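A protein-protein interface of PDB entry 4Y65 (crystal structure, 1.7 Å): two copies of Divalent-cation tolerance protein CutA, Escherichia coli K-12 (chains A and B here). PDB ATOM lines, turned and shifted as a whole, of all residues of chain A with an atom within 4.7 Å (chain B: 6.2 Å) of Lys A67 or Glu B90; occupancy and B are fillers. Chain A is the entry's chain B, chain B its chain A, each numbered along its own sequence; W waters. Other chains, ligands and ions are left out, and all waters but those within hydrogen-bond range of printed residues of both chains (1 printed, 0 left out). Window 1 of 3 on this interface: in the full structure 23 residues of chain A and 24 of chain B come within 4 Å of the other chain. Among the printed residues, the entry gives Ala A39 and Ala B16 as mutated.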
ATOM      1  N   VAL A  12      17.287   8.423   4.613  1.00  0.00           N
ATOM      2  CA  VAL A  12      18.547   7.700   4.529  1.00  0.00           C
ATOM      3  C   VAL A  12      19.623   8.523   5.221  1.00  0.00           C
ATOM      4  O   VAL A  12      19.431   9.707   5.519  1.00  0.00           O
ATOM      5  CB  VAL A  12      19.000   7.468   3.056  1.00  0.00           C
ATOM      6  CG1 VAL A  12      17.971   6.628   2.305  1.00  0.00           C
ATOM      7  CG2 VAL A  12      19.209   8.810   2.351  1.00  0.00           C
ATOM      8  N   VAL A  13      20.752   7.879   5.482  1.00  0.00           N
ATOM      9  CA  VAL A  13      21.890   8.529   6.113  1.00  0.00           C
ATOM     10  C   VAL A  13      23.047   8.424   5.134  1.00  0.00           C
ATOM     11  O   VAL A  13      23.280   7.363   4.559  1.00  0.00           O
ATOM     12  CB  VAL A  13      22.273   7.827   7.441  1.00  0.00           C
ATOM     13  CG1 VAL A  13      23.641   8.290   7.909  1.00  0.00           C
ATOM     14  CG2 VAL A  13      21.227   8.148   8.508  1.00  0.00           C
ATOM     15  N   ALA A  37      19.999  18.174   1.962  1.00  0.00           N
ATOM     16  CA  ALA A  37      20.125  17.424   3.205  1.00  0.00           C
ATOM     17  C   ALA A  37      19.399  18.248   4.263  1.00  0.00           C
ATOM     18  O   ALA A  37      19.312  19.469   4.142  1.00  0.00           O
ATOM     19  CB  ALA A  37      21.593  17.252   3.585  1.00  0.00           C
ATOM     20  N   ALA A  38      18.883  17.579   5.292  1.00  0.00           N
ATOM     21  CA  ALA A  38      18.166  18.253   6.370  1.00  0.00           C
ATOM     22  C   ALA A  38      19.091  18.584   7.534  1.00  0.00           C
ATOM     23  O   ALA A  38      18.863  19.547   8.262  1.00  0.00           O
ATOM     24  CB  ALA A  38      17.019  17.369   6.861  1.00  0.00           C
ATOM     25  N   ALA A  39      20.130  17.775   7.711  1.00  0.00           N
ATOM     26  CA  ALA A  39      21.076  17.988   8.801  1.00  0.00           C
ATOM     27  C   ALA A  39      22.392  17.281   8.518  1.00  0.00           C
ATOM     28  O   ALA A  39      22.442  16.327   7.740  1.00  0.00           O
ATOM     29  CB  ALA A  39      20.478  17.476  10.116  1.00  0.00           C
ATOM     30  N   ALA A  40      23.459  17.756   9.156  1.00  0.00           N
ATOM     31  CA  ALA A  40      24.781  17.169   8.986  1.00  0.00           C
ATOM     32  C   ALA A  40      25.500  17.138  10.322  1.00  0.00           C
ATOM     33  O   ALA A  40      25.501  18.126  11.056  1.00  0.00           O
ATOM     34  CB  ALA A  40      25.595  17.983   7.982  1.00  0.00           C
ATOM     35  N   THR A  41      26.087  15.991  10.639  1.00  0.00           N
ATOM     36  CA  THR A  41      26.851  15.828  11.866  1.00  0.00           C
ATOM     37  C   THR A  41      28.288  15.635  11.418  1.00  0.00           C
ATOM     38  O   THR A  41      28.565  14.805  10.545  1.00  0.00           O
ATOM     39  CB  THR A  41      26.405  14.582  12.658  1.00  0.00           C
ATOM     40  OG1 THR A  41      25.054  14.759  13.092  1.00  0.00           O
ATOM     41  CG2 THR A  41      27.307  14.369  13.871  1.00  0.00           C
ATOM     42  N   ILE A  65      28.056  12.708   8.657  1.00  0.00           N
ATOM     43  CA  ILE A  65      26.842  11.893   8.652  1.00  0.00           C
ATOM     44  C   ILE A  65      25.710  12.848   8.276  1.00  0.00           C
ATOM     45  O   ILE A  65      25.308  13.698   9.080  1.00  0.00           O
ATOM     46  CB  ILE A  65      26.558  11.288  10.052  1.00  0.00           C
ATOM     47  CG1 ILE A  65      27.770  10.486  10.535  1.00  0.00           C
ATOM     48  CG2 ILE A  65      25.325  10.396   9.985  1.00  0.00           C
ATOM     49  CD1 ILE A  65      27.614   9.931  11.952  1.00  0.00           C
ATOM     50  N   LEU A  66      25.215  12.736   7.047  1.00  0.00           N
ATOM     51  CA  LEU A  66      24.150  13.620   6.592  1.00  0.00           C
ATOM     52  C   LEU A  66      22.829  12.881   6.495  1.00  0.00           C
ATOM     53  O   LEU A  66      22.795  11.682   6.222  1.00  0.00           O
ATOM     54  CB  LEU A  66      24.505  14.244   5.234  1.00  0.00           C
ATOM     55  CG  LEU A  66      25.828  15.015   5.206  1.00  0.00           C
ATOM     56  CD1 LEU A  66      26.941  14.086   4.752  1.00  0.00           C
ATOM     57  CD2 LEU A  66      25.722  16.193   4.254  1.00  0.00           C
ATOM     58  N   LYS A  67      21.742  13.604   6.743  1.00  0.00           N
ATOM     59  CA  LYS A  67      20.402  13.033   6.702  1.00  0.00           C
ATOM     60  C   LYS A  67      19.643  13.590   5.512  1.00  0.00           C
ATOM     61  O   LYS A  67      19.594  14.803   5.318  1.00  0.00           O
ATOM     62  CB  LYS A  67      19.640  13.365   7.995  1.00  0.00           C
ATOM     63  CG  LYS A  67      19.898  12.411   9.160  1.00  0.00           C
ATOM     64  CD  LYS A  67      21.368  12.352   9.542  1.00  0.00           C
ATOM     65  CE  LYS A  67      21.875  13.656  10.128  1.00  0.00           C
ATOM     66  NZ  LYS A  67      21.214  13.984  11.411  1.00  0.00           N
ATOM     67  N   THR A  68      19.067  12.701   4.711  1.00  0.00           N
ATOM     68  CA  THR A  68      18.286  13.124   3.550  1.00  0.00           C
ATOM     69  C   THR A  68      17.279  12.020   3.231  1.00  0.00           C
ATOM     70  O   THR A  68      16.942  11.224   4.111  1.00  0.00           O
ATOM     71  CB  THR A  68      19.204  13.401   2.331  1.00  0.00           C
ATOM     72  OG1 THR A  68      18.446  14.048   1.297  1.00  0.00           O
ATOM     73  CG2 THR A  68      19.807  12.106   1.791  1.00  0.00           C
ATOM     74  N   TYR A 103      10.747  13.883  14.205  1.00  0.00           N
ATOM     75  CA  TYR A 103      12.026  14.167  13.580  1.00  0.00           C
ATOM     76  C   TYR A 103      11.955  13.920  12.077  1.00  0.00           C
ATOM     77  O   TYR A 103      12.465  14.712  11.288  1.00  0.00           O
ATOM     78  CB  TYR A 103      13.133  13.302  14.183  1.00  0.00           C
ATOM     79  CG  TYR A 103      14.493  13.602  13.593  1.00  0.00           C
ATOM     80  CD1 TYR A 103      15.144  14.801  13.872  1.00  0.00           C
ATOM     81  CD2 TYR A 103      15.106  12.713  12.713  1.00  0.00           C
ATOM     82  CE1 TYR A 103      16.366  15.113  13.287  1.00  0.00           C
ATOM     83  CE2 TYR A 103      16.333  13.017  12.118  1.00  0.00           C
ATOM     84  CZ  TYR A 103      16.955  14.220  12.414  1.00  0.00           C
ATOM     85  OH  TYR A 103      18.167  14.533  11.841  1.00  0.00           O
ATOM     86  N   LEU A 107      12.545  16.430   9.018  1.00  0.00           N
ATOM     87  CA  LEU A 107      13.557  16.086   8.028  1.00  0.00           C
ATOM     88  C   LEU A 107      12.962  16.205   6.624  1.00  0.00           C
ATOM     89  O   LEU A 107      13.555  16.818   5.737  1.00  0.00           O
ATOM     90  CB  LEU A 107      14.070  14.660   8.277  1.00  0.00           C
ATOM     91  CG  LEU A 107      15.150  14.072   7.363  1.00  0.00           C
ATOM     92  CD1 LEU A 107      15.805  12.888   8.061  1.00  0.00           C
ATOM     93  CD2 LEU A 107      14.541  13.637   6.034  1.00  0.00           C
ATOM     94  N   LEU B  15      20.717   5.875  15.919  1.00  0.00           N
ATOM     95  CA  LEU B  15      21.543   7.070  15.978  1.00  0.00           C
ATOM     96  C   LEU B  15      20.717   8.124  16.703  1.00  0.00           C
ATOM     97  O   LEU B  15      19.550   8.343  16.378  1.00  0.00           O
ATOM     98  CB  LEU B  15      21.883   7.582  14.572  1.00  0.00           C
ATOM     99  CG  LEU B  15      22.672   6.702  13.595  1.00  0.00           C
ATOM    100  CD1 LEU B  15      22.848   7.460  12.277  1.00  0.00           C
ATOM    101  CD2 LEU B  15      24.028   6.337  14.176  1.00  0.00           C
ATOM    102  N   ALA B  16      21.323   8.764  17.692  1.00  0.00           N
ATOM    103  CA  ALA B  16      20.668   9.819  18.452  1.00  0.00           C
ATOM    104  C   ALA B  16      21.778  10.761  18.865  1.00  0.00           C
ATOM    105  O   ALA B  16      22.925  10.341  18.976  1.00  0.00           O
ATOM    106  CB  ALA B  16      19.992   9.248  19.689  1.00  0.00           C
ATOM    107  N   THR B  17      21.451  12.029  19.082  1.00  0.00           N
ATOM    108  CA  THR B  17      22.463  12.981  19.516  1.00  0.00           C
ATOM    109  C   THR B  17      22.015  13.609  20.826  1.00  0.00           C
ATOM    110  O   THR B  17      20.821  13.795  21.055  1.00  0.00           O
ATOM    111  CB  THR B  17      22.695  14.104  18.477  1.00  0.00           C
ATOM    112  OG1 THR B  17      21.576  14.996  18.470  1.00  0.00           O
ATOM    113  CG2 THR B  17      22.871  13.515  17.094  1.00  0.00           C
ATOM    114  N   SER B  48      26.929  19.618  14.896  1.00  0.00           N
ATOM    115  CA  SER B  48      25.684  19.400  14.171  1.00  0.00           C
ATOM    116  C   SER B  48      25.218  20.686  13.508  1.00  0.00           C
ATOM    117  O   SER B  48      25.138  21.727  14.152  1.00  0.00           O
ATOM    118  CB  SER B  48      24.596  18.904  15.122  1.00  0.00           C
ATOM    119  OG  SER B  48      24.942  17.646  15.672  1.00  0.00           O
ATOM    120  N   GLN B  63      27.511  12.242  19.644  1.00  0.00           N
ATOM    121  CA  GLN B  63      26.826  11.298  18.765  1.00  0.00           C
ATOM    122  C   GLN B  63      26.678   9.981  19.508  1.00  0.00           C
ATOM    123  O   GLN B  63      27.665   9.421  19.987  1.00  0.00           O
ATOM    124  CB  GLN B  63      27.618  11.048  17.483  1.00  0.00           C
ATOM    125  CG  GLN B  63      26.958  10.010  16.565  1.00  0.00           C
ATOM    126  CD  GLN B  63      25.678  10.522  15.925  1.00  0.00           C
ATOM    127  OE1 GLN B  63      25.710  11.454  15.120  1.00  0.00           O
ATOM    128  NE2 GLN B  63      24.541   9.917  16.283  1.00  0.00           N
ATOM    129  N   MET B  64      25.448   9.492  19.606  1.00  0.00           N
ATOM    130  CA  MET B  64      25.193   8.227  20.290  1.00  0.00           C
ATOM    131  C   MET B  64      24.865   7.154  19.262  1.00  0.00           C
ATOM    132  O   MET B  64      24.186   7.427  18.273  1.00  0.00           O
ATOM    133  CB  MET B  64      24.006   8.361  21.249  1.00  0.00           C
ATOM    134  CG  MET B  64      24.154   9.453  22.301  1.00  0.00           C
ATOM    135  SD  MET B  64      22.673   9.600  23.315  1.00  0.00           S
ATOM    136  CE  MET B  64      22.895   8.188  24.388  1.00  0.00           C
ATOM    137  N   HIS B  84      14.744  13.055  26.599  1.00  0.00           N
ATOM    138  CA  HIS B  84      15.623  13.980  25.888  1.00  0.00           C
ATOM    139  C   HIS B  84      15.292  15.449  26.158  1.00  0.00           C
ATOM    140  O   HIS B  84      14.125  15.845  26.148  1.00  0.00           O
ATOM    141  CB  HIS B  84      15.546  13.713  24.385  1.00  0.00           C
ATOM    142  CG  HIS B  84      16.802  14.054  23.647  1.00  0.00           C
ATOM    143  ND1 HIS B  84      17.254  15.348  23.492  1.00  0.00           N
ATOM    144  CD2 HIS B  84      17.706  13.262  23.025  1.00  0.00           C
ATOM    145  CE1 HIS B  84      18.382  15.335  22.805  1.00  0.00           C
ATOM    146  NE2 HIS B  84      18.678  14.082  22.510  1.00  0.00           N
ATOM    147  N   TYR B  86      15.774  17.811  24.261  1.00  0.00           N
ATOM    148  CA  TYR B  86      15.433  18.450  22.991  1.00  0.00           C
ATOM    149  C   TYR B  86      13.963  18.211  22.673  1.00  0.00           C
ATOM    150  O   TYR B  86      13.360  17.245  23.151  1.00  0.00           O
ATOM    151  CB  TYR B  86      16.278  17.883  21.846  1.00  0.00           C
ATOM    152  CG  TYR B  86      17.719  18.345  21.809  1.00  0.00           C
ATOM    153  CD1 TYR B  86      18.368  18.778  22.965  1.00  0.00           C
ATOM    154  CD2 TYR B  86      18.453  18.290  20.622  1.00  0.00           C
ATOM    155  CE1 TYR B  86      19.711  19.141  22.942  1.00  0.00           C
ATOM    156  CE2 TYR B  86      19.795  18.648  20.588  1.00  0.00           C
ATOM    157  CZ  TYR B  86      20.419  19.071  21.751  1.00  0.00           C
ATOM    158  OH  TYR B  86      21.751  19.412  21.717  1.00  0.00           O
ATOM    159  N   THR B  88      12.660  17.982  19.358  1.00  0.00           N
ATOM    160  CA  THR B  88      12.612  17.027  18.253  1.00  0.00           C
ATOM    161  C   THR B  88      14.004  16.452  18.021  1.00  0.00           C
ATOM    162  O   THR B  88      14.640  16.738  17.009  1.00  0.00           O
ATOM    163  CB  THR B  88      12.162  17.721  16.962  1.00  0.00           C
ATOM    164  OG1 THR B  88      11.090  18.622  17.262  1.00  0.00           O
ATOM    165  CG2 THR B  88      11.686  16.697  15.939  1.00  0.00           C
ATOM    166  N   PRO B  89      14.490  15.624  18.955  1.00  0.00           N
ATOM    167  CA  PRO B  89      15.820  15.029  18.822  1.00  0.00           C
ATOM    168  C   PRO B  89      15.962  14.055  17.662  1.00  0.00           C
ATOM    169  O   PRO B  89      14.994  13.431  17.228  1.00  0.00           O
ATOM    170  CB  PRO B  89      16.021  14.345  20.168  1.00  0.00           C
ATOM    171  CG  PRO B  89      14.640  13.887  20.500  1.00  0.00           C
ATOM    172  CD  PRO B  89      13.811  15.111  20.159  1.00  0.00           C
ATOM    173  N   GLU B  90      17.183  13.943  17.161  1.00  0.00           N
ATOM    174  CA  GLU B  90      17.476  13.022  16.075  1.00  0.00           C
ATOM    175  C   GLU B  90      17.346  11.621  16.648  1.00  0.00           C
ATOM    176  O   GLU B  90      17.986  11.293  17.645  1.00  0.00           O
ATOM    177  CB  GLU B  90      18.904  13.237  15.566  1.00  0.00           C
ATOM    178  CG  GLU B  90      19.446  12.087  14.722  1.00  0.00           C
ATOM    179  CD  GLU B  90      20.954  12.151  14.556  1.00  0.00           C
ATOM    180  OE1 GLU B  90      21.445  13.133  13.961  1.00  0.00           O
ATOM    181  OE2 GLU B  90      21.649  11.220  15.028  1.00  0.00           O
ATOM    182  N   LEU B  91      16.502  10.803  16.028  1.00  0.00           N
ATOM    183  CA  LEU B  91      16.300   9.429  16.463  1.00  0.00           C
ATOM    184  C   LEU B  91      16.034   8.626  15.201  1.00  0.00           C
ATOM    185  O   LEU B  91      14.930   8.661  14.653  1.00  0.00           O
ATOM    186  CB  LEU B  91      15.110   9.327  17.421  1.00  0.00           C
ATOM    187  CG  LEU B  91      15.273  10.011  18.785  1.00  0.00           C
ATOM    188  CD1 LEU B  91      13.955   9.995  19.544  1.00  0.00           C
ATOM    189  CD2 LEU B  91      16.350   9.293  19.582  1.00  0.00           C
ATOM    190  N   LEU B  92      17.059   7.914  14.743  1.00  0.00           N
ATOM    191  CA  LEU B  92      16.970   7.127  13.521  1.00  0.00           C
ATOM    192  C   LEU B  92      17.399   5.685  13.742  1.00  0.00           C
ATOM    193  O   LEU B  92      18.300   5.413  14.534  1.00  0.00           O
ATOM    194  CB  LEU B  92      17.855   7.764  12.448  1.00  0.00           C
ATOM    195  CG  LEU B  92      17.530   9.217  12.094  1.00  0.00           C
ATOM    196  CD1 LEU B  92      18.671   9.807  11.277  1.00  0.00           C
ATOM    197  CD2 LEU B  92      16.208   9.281  11.319  1.00  0.00           C
HETATM  198  O   HOH W   1      23.899  11.655  13.305  1.00  0.00           O
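Among the printed residues, pairs that only touch across the chains: Ala A40 with Ser B48 (3.4 Å), Thr A41 with Ser B48 (3.9 Å), Thr A41 with Gln B63 (3.6 Å), Ile A65 with Gln B63 (3.998 Å), Lys A67 with Leu B92 (3.6 Å), Tyr A103 with Thr B88 (3.4 Å), Tyr A103 with Pro B89 (3.6 Å), Tyr A103 with Glu B90 (3.7 Å) and Tyr A103 with Leu B92 (3.8 Å).
Water W1 lies within hydrogen-bond range of OE1 of Gln B63 (2.6 Å), OE2 of Glu B90 (2.9 Å) and OG1 of Thr A41 (3.3 Å).
The backbone NH (N) of Leu B15 is in hydrogen-bond range of the backbone carbonyl oxygen (O) of Leu B92 (2.8 Å). The side-chain amide nitrogen (NE2) of Gln B63 lies within hydrogen-bond range of the backbone carbonyl oxygen (O) of Ala B16. The side-chain amide nitrogen (NE2) of Gln B63 is in hydrogen-bond range of the side-chain carboxylate (OE2) of Glu B90, 3.4 Å away. N of Lys A67 sits at hydrogen-bond distance from O of Ala A39 (3.0 Å). O of Thr A41 sits at hydrogen-bond distance from N of Ile A65 (2.9 Å). The side-chain amino group (NZ) of Lys A67 is in hydrogen-bond range of the side-chain hydroxyl (OH) of Tyr A103 (3.1 Å).
No position is printed for both chains. Of the 10 pairs that touch across the chains among the printed residues, none has its exchanged pair printed and touching as well.
NZ of Lys A67 lies within salt-bridge range of OE1 of Glu B90, at 2.7 Å.
Lys A67 touches just these residues of chain B: Glu B90 and Leu B92. Of chain A, only Lys A67 and Tyr A103 come within 4 Å of Glu B90. Printed residues of chain A within 4 Å of Pro B89: Tyr A103. Printed residues of chain B within 4 Å of Ile A65: Gln B63. Printed residues of chain A within 4 Å of Thr B88: Tyr A103 (3.4 Å). Ala B16 touches none of the printed residues of chain A. The nearest residue of chain B that does not touch Lys A67 is Leu B15 (5.8 Å). The nearest printed residue of chain A that does not touch Leu B92 is Val A13 (4.1 Å).
Of the 13 printed residues of chain A, 5 touch a printed residue of chain B. Printed residues of chain A that touch a printed residue of chain B: Ala A40, Thr A41, Ile A65, Lys A67 and Tyr A103. Of the 13 printed residues of chain B, 6 touch a printed residue of chain A. Among the printed residues, Asp or Glu carboxylates within 4 Å of a Lys or Arg side-chain nitrogen of the other chain: Lys A67 with Glu B90.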
